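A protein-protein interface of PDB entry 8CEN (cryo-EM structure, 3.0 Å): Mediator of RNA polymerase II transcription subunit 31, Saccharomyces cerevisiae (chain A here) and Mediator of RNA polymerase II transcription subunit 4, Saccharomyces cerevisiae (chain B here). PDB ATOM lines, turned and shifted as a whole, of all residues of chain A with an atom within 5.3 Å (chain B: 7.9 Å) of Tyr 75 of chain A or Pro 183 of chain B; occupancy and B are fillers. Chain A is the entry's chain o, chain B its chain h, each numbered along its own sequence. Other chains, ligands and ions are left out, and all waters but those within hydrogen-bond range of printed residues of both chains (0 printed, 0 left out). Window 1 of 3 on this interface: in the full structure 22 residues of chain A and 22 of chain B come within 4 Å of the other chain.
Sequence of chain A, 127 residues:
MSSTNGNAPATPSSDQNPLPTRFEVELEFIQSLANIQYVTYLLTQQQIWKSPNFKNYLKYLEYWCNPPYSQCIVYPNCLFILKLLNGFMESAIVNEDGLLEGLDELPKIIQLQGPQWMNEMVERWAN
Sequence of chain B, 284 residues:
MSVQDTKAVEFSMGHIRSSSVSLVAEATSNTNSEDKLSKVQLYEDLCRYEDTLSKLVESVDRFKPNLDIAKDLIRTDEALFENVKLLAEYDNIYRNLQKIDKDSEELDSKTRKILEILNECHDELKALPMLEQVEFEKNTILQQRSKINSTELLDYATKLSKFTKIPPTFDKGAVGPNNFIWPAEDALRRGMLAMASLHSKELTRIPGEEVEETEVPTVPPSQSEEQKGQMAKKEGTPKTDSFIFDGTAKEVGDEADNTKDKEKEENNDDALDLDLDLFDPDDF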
ATOM      1  N   GLN A  31      19.205  10.738  -5.397  1.00  0.00           N
ATOM      2  CA  GLN A  31      18.935  11.915  -6.207  1.00  0.00           C
ATOM      3  C   GLN A  31      18.039  11.594  -7.392  1.00  0.00           C
ATOM      4  O   GLN A  31      17.328  12.479  -7.878  1.00  0.00           O
ATOM      5  CB  GLN A  31      20.244  12.541  -6.675  1.00  0.00           C
ATOM      6  CG  GLN A  31      20.957  13.285  -5.569  1.00  0.00           C
ATOM      7  CD  GLN A  31      21.773  14.439  -6.077  1.00  0.00           C
ATOM      8  OE1 GLN A  31      21.310  15.572  -6.079  1.00  0.00           O
ATOM      9  NE2 GLN A  31      22.990  14.161  -6.522  1.00  0.00           N
ATOM     10  N   SER A  32      18.039  10.339  -7.850  1.00  0.00           N
ATOM     11  CA  SER A  32      17.126   9.913  -8.904  1.00  0.00           C
ATOM     12  C   SER A  32      15.662   9.953  -8.481  1.00  0.00           C
ATOM     13  O   SER A  32      14.785   9.886  -9.350  1.00  0.00           O
ATOM     14  CB  SER A  32      17.494   8.503  -9.361  1.00  0.00           C
ATOM     15  OG  SER A  32      17.323   7.575  -8.307  1.00  0.00           O
ATOM     16  N   ALA A  34      14.195  12.537  -7.406  1.00  0.00           N
ATOM     17  CA  ALA A  34      13.667  13.775  -7.967  1.00  0.00           C
ATOM     18  C   ALA A  34      13.067  13.533  -9.343  1.00  0.00           C
ATOM     19  O   ALA A  34      12.042  14.128  -9.698  1.00  0.00           O
ATOM     20  CB  ALA A  34      14.764  14.835  -8.044  1.00  0.00           C
ATOM     21  N   ASN A  35      13.700  12.674 -10.137  1.00  0.00           N
ATOM     22  CA  ASN A  35      13.104  12.217 -11.387  1.00  0.00           C
ATOM     23  C   ASN A  35      11.926  11.324 -11.039  1.00  0.00           C
ATOM     24  O   ASN A  35      12.107  10.179 -10.614  1.00  0.00           O
ATOM     25  CB  ASN A  35      14.138  11.479 -12.232  1.00  0.00           C
ATOM     26  CG  ASN A  35      13.698  11.299 -13.674  1.00  0.00           C
ATOM     27  OD1 ASN A  35      12.566  11.615 -14.037  1.00  0.00           O
ATOM     28  ND2 ASN A  35      14.599  10.793 -14.505  1.00  0.00           N
ATOM     29  N   ILE A  73      23.591  16.956  -1.756  1.00  0.00           N
ATOM     30  CA  ILE A  73      22.356  16.773  -2.511  1.00  0.00           C
ATOM     31  C   ILE A  73      22.221  17.930  -3.494  1.00  0.00           C
ATOM     32  O   ILE A  73      21.994  19.075  -3.099  1.00  0.00           O
ATOM     33  CB  ILE A  73      21.135  16.684  -1.590  1.00  0.00           C
ATOM     34  CG1 ILE A  73      21.275  15.496  -0.637  1.00  0.00           C
ATOM     35  CG2 ILE A  73      19.870  16.558  -2.413  1.00  0.00           C
ATOM     36  CD1 ILE A  73      21.258  14.154  -1.334  1.00  0.00           C
ATOM     37  N   VAL A  74      22.355  17.626  -4.782  1.00  0.00           N
ATOM     38  CA  VAL A  74      22.276  18.648  -5.817  1.00  0.00           C
ATOM     39  C   VAL A  74      20.824  18.932  -6.189  1.00  0.00           C
ATOM     40  O   VAL A  74      20.469  20.074  -6.506  1.00  0.00           O
ATOM     41  CB  VAL A  74      23.114  18.186  -7.023  1.00  0.00           C
ATOM     42  CG1 VAL A  74      23.006  19.143  -8.185  1.00  0.00           C
ATOM     43  CG2 VAL A  74      24.561  18.004  -6.605  1.00  0.00           C
ATOM     44  N   TYR A  75      19.957  17.920  -6.121  1.00  0.00           N
ATOM     45  CA  TYR A  75      18.557  18.020  -6.529  1.00  0.00           C
ATOM     46  C   TYR A  75      17.652  17.768  -5.325  1.00  0.00           C
ATOM     47  O   TYR A  75      17.075  16.682  -5.207  1.00  0.00           O
ATOM     48  CB  TYR A  75      18.238  17.019  -7.638  1.00  0.00           C
ATOM     49  CG  TYR A  75      19.197  16.992  -8.811  1.00  0.00           C
ATOM     50  CD1 TYR A  75      19.132  17.954  -9.807  1.00  0.00           C
ATOM     51  CD2 TYR A  75      20.135  15.977  -8.944  1.00  0.00           C
ATOM     52  CE1 TYR A  75      19.993  17.925 -10.887  1.00  0.00           C
ATOM     53  CE2 TYR A  75      21.002  15.940 -10.020  1.00  0.00           C
ATOM     54  CZ  TYR A  75      20.925  16.917 -10.988  1.00  0.00           C
ATOM     55  OH  TYR A  75      21.783  16.885 -12.062  1.00  0.00           O
ATOM     56  N   PRO A  76      17.448  18.767  -4.456  1.00  0.00           N
ATOM     57  CA  PRO A  76      16.786  18.517  -3.155  1.00  0.00           C
ATOM     58  C   PRO A  76      15.324  18.084  -3.242  1.00  0.00           C
ATOM     59  O   PRO A  76      14.777  17.554  -2.254  1.00  0.00           O
ATOM     60  CB  PRO A  76      16.910  19.866  -2.438  1.00  0.00           C
ATOM     61  CG  PRO A  76      17.880  20.681  -3.248  1.00  0.00           C
ATOM     62  CD  PRO A  76      17.775  20.187  -4.644  1.00  0.00           C
ATOM     63  N   ASN A  77      14.675  18.259  -4.392  1.00  0.00           N
ATOM     64  CA  ASN A  77      13.343  17.696  -4.563  1.00  0.00           C
ATOM     65  C   ASN A  77      13.360  16.174  -4.492  1.00  0.00           C
ATOM     66  O   ASN A  77      12.320  15.566  -4.229  1.00  0.00           O
ATOM     67  CB  ASN A  77      12.741  18.188  -5.878  1.00  0.00           C
ATOM     68  CG  ASN A  77      12.458  19.678  -5.854  1.00  0.00           C
ATOM     69  OD1 ASN A  77      12.521  20.310  -4.804  1.00  0.00           O
ATOM     70  ND2 ASN A  77      12.132  20.240  -7.002  1.00  0.00           N
ATOM     71  N   CYS A  78      14.530  15.553  -4.672  1.00  0.00           N
ATOM     72  CA  CYS A  78      14.675  14.132  -4.382  1.00  0.00           C
ATOM     73  C   CYS A  78      14.468  13.849  -2.903  1.00  0.00           C
ATOM     74  O   CYS A  78      13.848  12.846  -2.540  1.00  0.00           O
ATOM     75  CB  CYS A  78      16.056  13.644  -4.789  1.00  0.00           C
ATOM     76  SG  CYS A  78      17.380  14.059  -3.619  1.00  0.00           S
ATOM     77  N   LEU A  79      15.018  14.703  -2.032  1.00  0.00           N
ATOM     78  CA  LEU A  79      14.776  14.565  -0.598  1.00  0.00           C
ATOM     79  C   LEU A  79      13.303  14.764  -0.276  1.00  0.00           C
ATOM     80  O   LEU A  79      12.745  14.067   0.585  1.00  0.00           O
ATOM     81  CB  LEU A  79      15.624  15.564   0.188  1.00  0.00           C
ATOM     82  CG  LEU A  79      17.132  15.348   0.248  1.00  0.00           C
ATOM     83  CD1 LEU A  79      17.821  16.620   0.704  1.00  0.00           C
ATOM     84  CD2 LEU A  79      17.449  14.203   1.183  1.00  0.00           C
ATOM     85  N   TYR B 156      26.287  25.368   0.608  1.00  0.00           N
ATOM     86  CA  TYR B 156      25.200  24.606   0.006  1.00  0.00           C
ATOM     87  C   TYR B 156      24.396  25.460  -0.966  1.00  0.00           C
ATOM     88  O   TYR B 156      23.968  24.977  -2.021  1.00  0.00           O
ATOM     89  CB  TYR B 156      24.297  24.034   1.093  1.00  0.00           C
ATOM     90  CG  TYR B 156      23.284  23.056   0.561  1.00  0.00           C
ATOM     91  CD1 TYR B 156      23.642  22.108  -0.386  1.00  0.00           C
ATOM     92  CD2 TYR B 156      21.969  23.083   0.997  1.00  0.00           C
ATOM     93  CE1 TYR B 156      22.723  21.213  -0.880  1.00  0.00           C
ATOM     94  CE2 TYR B 156      21.043  22.191   0.509  1.00  0.00           C
ATOM     95  CZ  TYR B 156      21.423  21.257  -0.430  1.00  0.00           C
ATOM     96  OH  TYR B 156      20.500  20.364  -0.922  1.00  0.00           O
ATOM     97  N   LEU B 160      23.743  24.962  -4.945  1.00  0.00           N
ATOM     98  CA  LEU B 160      22.423  24.905  -5.566  1.00  0.00           C
ATOM     99  C   LEU B 160      22.132  26.074  -6.498  1.00  0.00           C
ATOM    100  O   LEU B 160      21.060  26.087  -7.112  1.00  0.00           O
ATOM    101  CB  LEU B 160      21.330  24.857  -4.498  1.00  0.00           C
ATOM    102  CG  LEU B 160      21.335  23.695  -3.510  1.00  0.00           C
ATOM    103  CD1 LEU B 160      20.187  23.863  -2.538  1.00  0.00           C
ATOM    104  CD2 LEU B 160      21.241  22.369  -4.237  1.00  0.00           C
ATOM    105  N   LYS B 162      23.416  26.969  -9.398  1.00  0.00           N
ATOM    106  CA  LYS B 162      23.378  26.641 -10.816  1.00  0.00           C
ATOM    107  C   LYS B 162      22.325  25.597 -11.166  1.00  0.00           C
ATOM    108  O   LYS B 162      22.186  25.252 -12.344  1.00  0.00           O
ATOM    109  CB  LYS B 162      24.754  26.152 -11.284  1.00  0.00           C
ATOM    110  CG  LYS B 162      25.135  26.637 -12.673  1.00  0.00           C
ATOM    111  CD  LYS B 162      26.255  25.805 -13.271  1.00  0.00           C
ATOM    112  CE  LYS B 162      27.610  26.430 -13.005  1.00  0.00           C
ATOM    113  NZ  LYS B 162      28.679  25.779 -13.810  1.00  0.00           N
ATOM    114  N   PHE B 163      21.576  25.092 -10.189  1.00  0.00           N
ATOM    115  CA  PHE B 163      20.646  23.997 -10.431  1.00  0.00           C
ATOM    116  C   PHE B 163      19.196  24.363 -10.157  1.00  0.00           C
ATOM    117  O   PHE B 163      18.334  24.137 -11.013  1.00  0.00           O
ATOM    118  CB  PHE B 163      21.051  22.782  -9.585  1.00  0.00           C
ATOM    119  CG  PHE B 163      22.296  22.104 -10.070  1.00  0.00           C
ATOM    120  CD1 PHE B 163      22.236  21.162 -11.083  1.00  0.00           C
ATOM    121  CD2 PHE B 163      23.530  22.428  -9.533  1.00  0.00           C
ATOM    122  CE1 PHE B 163      23.379  20.540 -11.537  1.00  0.00           C
ATOM    123  CE2 PHE B 163      24.681  21.810  -9.986  1.00  0.00           C
ATOM    124  CZ  PHE B 163      24.604  20.866 -10.990  1.00  0.00           C
ATOM    125  N   THR B 164      18.900  24.936  -8.991  1.00  0.00           N
ATOM    126  CA  THR B 164      17.521  25.052  -8.536  1.00  0.00           C
ATOM    127  C   THR B 164      16.723  26.142  -9.245  1.00  0.00           C
ATOM    128  O   THR B 164      15.509  26.226  -9.027  1.00  0.00           O
ATOM    129  CB  THR B 164      17.499  25.291  -7.028  1.00  0.00           C
ATOM    130  OG1 THR B 164      18.264  26.462  -6.722  1.00  0.00           O
ATOM    131  CG2 THR B 164      18.091  24.101  -6.295  1.00  0.00           C
ATOM    132  N   PRO B 177      14.026  21.672 -18.096  1.00  0.00           N
ATOM    133  CA  PRO B 177      14.123  21.294 -16.682  1.00  0.00           C
ATOM    134  C   PRO B 177      14.789  19.944 -16.471  1.00  0.00           C
ATOM    135  O   PRO B 177      14.670  19.347 -15.397  1.00  0.00           O
ATOM    136  CB  PRO B 177      12.656  21.262 -16.249  1.00  0.00           C
ATOM    137  CG  PRO B 177      11.941  20.846 -17.462  1.00  0.00           C
ATOM    138  CD  PRO B 177      12.679  21.423 -18.636  1.00  0.00           C
ATOM    139  N   ASN B 178      15.497  19.463 -17.495  1.00  0.00           N
ATOM    140  CA  ASN B 178      15.864  18.052 -17.569  1.00  0.00           C
ATOM    141  C   ASN B 178      16.952  17.683 -16.572  1.00  0.00           C
ATOM    142  O   ASN B 178      16.894  16.610 -15.964  1.00  0.00           O
ATOM    143  CB  ASN B 178      16.305  17.715 -18.987  1.00  0.00           C
ATOM    144  CG  ASN B 178      15.151  17.699 -19.947  1.00  0.00           C
ATOM    145  OD1 ASN B 178      14.912  18.676 -20.655  1.00  0.00           O
ATOM    146  ND2 ASN B 178      14.414  16.595 -19.970  1.00  0.00           N
ATOM    147  N   ASN B 179      17.965  18.533 -16.408  1.00  0.00           N
ATOM    148  CA  ASN B 179      19.061  18.238 -15.491  1.00  0.00           C
ATOM    149  C   ASN B 179      19.239  19.323 -14.437  1.00  0.00           C
ATOM    150  O   ASN B 179      20.327  19.462 -13.870  1.00  0.00           O
ATOM    151  CB  ASN B 179      20.362  18.020 -16.261  1.00  0.00           C
ATOM    152  CG  ASN B 179      20.377  16.707 -17.015  1.00  0.00           C
ATOM    153  OD1 ASN B 179      20.689  15.662 -16.451  1.00  0.00           O
ATOM    154  ND2 ASN B 179      20.040  16.755 -18.299  1.00  0.00           N
ATOM    155  N   PHE B 180      18.189  20.092 -14.160  1.00  0.00           N
ATOM    156  CA  PHE B 180      18.221  21.140 -13.150  1.00  0.00           C
ATOM    157  C   PHE B 180      17.448  20.755 -11.896  1.00  0.00           C
ATOM    158  O   PHE B 180      17.968  20.875 -10.783  1.00  0.00           O
ATOM    159  CB  PHE B 180      17.661  22.444 -13.728  1.00  0.00           C
ATOM    160  CG  PHE B 180      18.535  23.069 -14.777  1.00  0.00           C
ATOM    161  CD1 PHE B 180      18.475  22.647 -16.093  1.00  0.00           C
ATOM    162  CD2 PHE B 180      19.417  24.082 -14.444  1.00  0.00           C
ATOM    163  CE1 PHE B 180      19.275  23.221 -17.057  1.00  0.00           C
ATOM    164  CE2 PHE B 180      20.222  24.659 -15.405  1.00  0.00           C
ATOM    165  CZ  PHE B 180      20.148  24.231 -16.713  1.00  0.00           C
ATOM    166  N   ILE B 181      16.214  20.287 -12.055  1.00  0.00           N
ATOM    167  CA  ILE B 181      15.409  19.863 -10.916  1.00  0.00           C
ATOM    168  C   ILE B 181      15.729  18.425 -10.551  1.00  0.00           C
ATOM    169  O   ILE B 181      15.833  18.079  -9.374  1.00  0.00           O
ATOM    170  CB  ILE B 181      13.895  20.019 -11.193  1.00  0.00           C
ATOM    171  CG1 ILE B 181      13.472  21.461 -11.439  1.00  0.00           C
ATOM    172  CG2 ILE B 181      13.090  19.522 -10.034  1.00  0.00           C
ATOM    173  CD1 ILE B 181      13.549  21.854 -12.857  1.00  0.00           C
ATOM    174  N   TRP B 182      15.886  17.586 -11.561  1.00  0.00           N
ATOM    175  CA  TRP B 182      16.048  16.152 -11.408  1.00  0.00           C
ATOM    176  C   TRP B 182      17.169  15.693 -12.324  1.00  0.00           C
ATOM    177  O   TRP B 182      17.523  16.396 -13.274  1.00  0.00           O
ATOM    178  CB  TRP B 182      14.742  15.416 -11.737  1.00  0.00           C
ATOM    179  CG  TRP B 182      14.123  15.753 -13.065  1.00  0.00           C
ATOM    180  CD1 TRP B 182      14.565  15.376 -14.298  1.00  0.00           C
ATOM    181  CD2 TRP B 182      12.923  16.505 -13.286  1.00  0.00           C
ATOM    182  NE1 TRP B 182      13.731  15.864 -15.272  1.00  0.00           N
ATOM    183  CE2 TRP B 182      12.713  16.558 -14.676  1.00  0.00           C
ATOM    184  CE3 TRP B 182      12.010  17.142 -12.442  1.00  0.00           C
ATOM    185  CZ2 TRP B 182      11.629  17.226 -15.242  1.00  0.00           C
ATOM    186  CZ3 TRP B 182      10.936  17.807 -13.005  1.00  0.00           C
ATOM    187  CH2 TRP B 182      10.755  17.843 -14.391  1.00  0.00           C
ATOM    188  N   PRO B 183      17.773  14.539 -12.045  1.00  0.00           N
ATOM    189  CA  PRO B 183      18.669  13.929 -13.034  1.00  0.00           C
ATOM    190  C   PRO B 183      17.861  13.332 -14.178  1.00  0.00           C
ATOM    191  O   PRO B 183      16.904  12.587 -13.957  1.00  0.00           O
ATOM    192  CB  PRO B 183      19.403  12.846 -12.236  1.00  0.00           C
ATOM    193  CG  PRO B 183      18.518  12.553 -11.089  1.00  0.00           C
ATOM    194  CD  PRO B 183      17.815  13.831 -10.756  1.00  0.00           C
ATOM    195  N   ALA B 184      18.249  13.669 -15.403  1.00  0.00           N
ATOM    196  CA  ALA B 184      17.526  13.206 -16.576  1.00  0.00           C
ATOM    197  C   ALA B 184      17.839  11.737 -16.847  1.00  0.00           C
ATOM    198  O   ALA B 184      18.631  11.097 -16.145  1.00  0.00           O
ATOM    199  CB  ALA B 184      17.866  14.069 -17.787  1.00  0.00           C
ATOM    200  N   GLU B 185      17.195  11.199 -17.888  1.00  0.00           N
ATOM    201  CA  GLU B 185      17.430   9.814 -18.277  1.00  0.00           C
ATOM    202  C   GLU B 185      18.881   9.600 -18.673  1.00  0.00           C
ATOM    203  O   GLU B 185      19.516   8.640 -18.226  1.00  0.00           O
ATOM    204  CB  GLU B 185      16.501   9.417 -19.426  1.00  0.00           C
ATOM    205  CG  GLU B 185      16.286   7.909 -19.565  1.00  0.00           C
ATOM    206  CD  GLU B 185      17.329   7.220 -20.443  1.00  0.00           C
ATOM    207  OE1 GLU B 185      18.232   7.891 -20.970  1.00  0.00           O
ATOM    208  OE2 GLU B 185      17.260   5.988 -20.603  1.00  0.00           O
ATOM    209  N   ASP B 186      19.416  10.476 -19.531  1.00  0.00           N
ATOM    210  CA  ASP B 186      20.804  10.345 -19.959  1.00  0.00           C
ATOM    211  C   ASP B 186      21.762  10.503 -18.789  1.00  0.00           C
ATOM    212  O   ASP B 186      22.817   9.862 -18.764  1.00  0.00           O
ATOM    213  CB  ASP B 186      21.124  11.369 -21.046  1.00  0.00           C
ATOM    214  CG  ASP B 186      20.652  12.763 -20.690  1.00  0.00           C
ATOM    215  OD1 ASP B 186      19.437  12.936 -20.461  1.00  0.00           O
ATOM    216  OD2 ASP B 186      21.493  13.684 -20.634  1.00  0.00           O
ATOM    217  N   ALA B 187      21.399  11.338 -17.810  1.00  0.00           N
ATOM    218  CA  ALA B 187      22.188  11.450 -16.589  1.00  0.00           C
ATOM    219  C   ALA B 187      22.205  10.138 -15.819  1.00  0.00           C
ATOM    220  O   ALA B 187      23.252   9.726 -15.310  1.00  0.00           O
ATOM    221  CB  ALA B 187      21.644  12.575 -15.712  1.00  0.00           C
ATOM    222  N   LEU B 188      21.057   9.458 -15.730  1.00  0.00           N
ATOM    223  CA  LEU B 188      21.031   8.173 -15.035  1.00  0.00           C
ATOM    224  C   LEU B 188      21.754   7.082 -15.821  1.00  0.00           C
ATOM    225  O   LEU B 188      22.295   6.147 -15.222  1.00  0.00           O
ATOM    226  CB  LEU B 188      19.590   7.757 -14.742  1.00  0.00           C
ATOM    227  CG  LEU B 188      18.793   8.734 -13.876  1.00  0.00           C
ATOM    228  CD1 LEU B 188      17.336   8.317 -13.768  1.00  0.00           C
ATOM    229  CD2 LEU B 188      19.426   8.859 -12.501  1.00  0.00           C
ATOM    230  N   ARG B 189      21.770   7.181 -17.152  1.00  0.00           N
ATOM    231  CA  ARG B 189      22.486   6.199 -17.965  1.00  0.00           C
ATOM    232  C   ARG B 189      23.995   6.369 -17.838  1.00  0.00           C
ATOM    233  O   ARG B 189      24.708   5.427 -17.473  1.00  0.00           O
ATOM    234  CB  ARG B 189      22.074   6.311 -19.431  1.00  0.00           C
ATOM    235  CG  ARG B 189      20.610   6.113 -19.713  1.00  0.00           C
ATOM    236  CD  ARG B 189      20.184   4.656 -19.725  1.00  0.00           C
ATOM    237  NE  ARG B 189      20.488   3.990 -20.988  1.00  0.00           N
ATOM    238  CZ  ARG B 189      19.915   4.245 -22.158  1.00  0.00           C
ATOM    239  NH1 ARG B 189      18.965   5.157 -22.288  1.00  0.00           N
ATOM    240  NH2 ARG B 189      20.306   3.564 -23.231  1.00  0.00           N
ATOM    241  N   ARG B 190      24.506   7.565 -18.152  1.00  0.00           N
ATOM    242  CA  ARG B 190      25.942   7.802 -18.048  1.00  0.00           C
ATOM    243  C   ARG B 190      26.411   7.860 -16.604  1.00  0.00           C
ATOM    244  O   ARG B 190      27.621   7.807 -16.359  1.00  0.00           O
ATOM    245  CB  ARG B 190      26.345   9.100 -18.749  1.00  0.00           C
ATOM    246  CG  ARG B 190      25.881  10.359 -18.042  1.00  0.00           C
ATOM    247  CD  ARG B 190      26.301  11.609 -18.789  1.00  0.00           C
ATOM    248  NE  ARG B 190      25.890  12.817 -18.087  1.00  0.00           N
ATOM    249  CZ  ARG B 190      24.739  13.445 -18.288  1.00  0.00           C
ATOM    250  NH1 ARG B 190      23.865  13.016 -19.183  1.00  0.00           N
ATOM    251  NH2 ARG B 190      24.460  14.533 -17.575  1.00  0.00           N
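Of chain B, only Phe 163, Asn 179, Phe 180, Ile 181, Trp 182 and Pro 183 come within 4 Å of Tyr 75 of chain A. Of the printed residues of chain A, Pro 183 of chain B touches Gln 31, Ser 32, Asn 35 and Tyr 75. Pro 76 of chain A touches two residues of chain B. Of the printed residues of chain B, Ile 73 of chain A touches Tyr 156 and Leu 160. Of the printed residues of chain B, Ala 34 of chain A touches Ile 181 (3.7 Å) and Trp 182 (3.5 Å). Printed residues of chain A within 4 Å of Asn 179 of chain B: Tyr 75. Printed residues of chain A within 4 Å of Phe 163 of chain B: Val 74 (3.6 Å) and Tyr 75 (3.9 Å). Thr 164 of chain B touches none of the printed residues of chain A. The nearest residue of chain B that does not touch Tyr 75 of chain A is Leu 160 of chain B (5.0 Å). The nearest printed residue of chain B that does not touch Ser 32 of chain A is Trp 182 of chain B (6.0 Å).
Pro 183 of chain B touches Gln 31 of chain A. CB of Trp 182 of chain B touches N of Asn 35 of chain A (3.3 Å). Asn 35 of chain A touches Leu 188 of chain B (ND2 to CD1, 3.8 Å). Leu 160 of chain B touches Ile 73 of chain A (CD2 to O, 3.6 Å). Val 74 of chain A touches Leu 160 of chain B (O to CD2, 3.3 Å). CG1 of Val 74 of chain A touches CG of Phe 163 of chain B, at 3.6 Å. Phe 180 of chain B touches Tyr 75 of chain A (O to CD1, 3.3 Å). Trp 182 of chain B touches Tyr 75 of chain A (N to CD1, 3.7 Å). Tyr 156 of chain B touches Pro 76 of chain A. Asn 77 of chain A touches Ile 181 of chain B.
The side-chain hydroxyl of Tyr 156 of chain B is in hydrogen-bond range of the backbone carbonyl oxygen of Ile 73 of chain A, at 2.9 Å. The backbone carbonyl oxygen of Asn 179 of chain B lies close to the side-chain hydroxyl of Tyr 75 of chain A. O of Pro 183 of chain B lies within hydrogen-bond range of ND2 of Asn 35 of chain A (3.0 Å).
Hydrophobic or aromatic side chains of chain A that line the printed part of chain B: Ala 34, Ile 73, Val 74, Tyr 75 and Pro 76. Of the 19 printed residues of chain B, 9 touch a printed residue of chain A. Hydrophobic or aromatic side chains of chain B within 4 Å of the printed part of chain A: Tyr 156, Leu 160, Phe 163, Ile 181, Trp 182, Pro 183 and Leu 188. Among the printed residues, 21 pairs touch across the chains.
O of Tyr 75 of chain A lies within hydrogen-bond range of SG of Cys 78 of chain A, 3.1 Å away. O of Leu 160 of chain B is in hydrogen-bond range of OG1 of Thr 164 of chain B, 2.8 Å away. NE1 of Trp 182 of chain B lies close to O of Asn 178 of chain B (3.3 Å). The backbone NH (N) of Ala 184 of chain B lies within hydrogen-bond range of the side-chain amide oxygen (OD1) of Asn 179 of chain B (3.3 Å). The side-chain amide oxygen (OE1) of Gln 31 of chain A is in hydrogen-bond range of the backbone NH (N) of Tyr 75 of chain A (2.7 Å). N of Val 74 of chain A sits at hydrogen-bond distance from OE1 of Gln 31 of chain A (2.6 Å).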
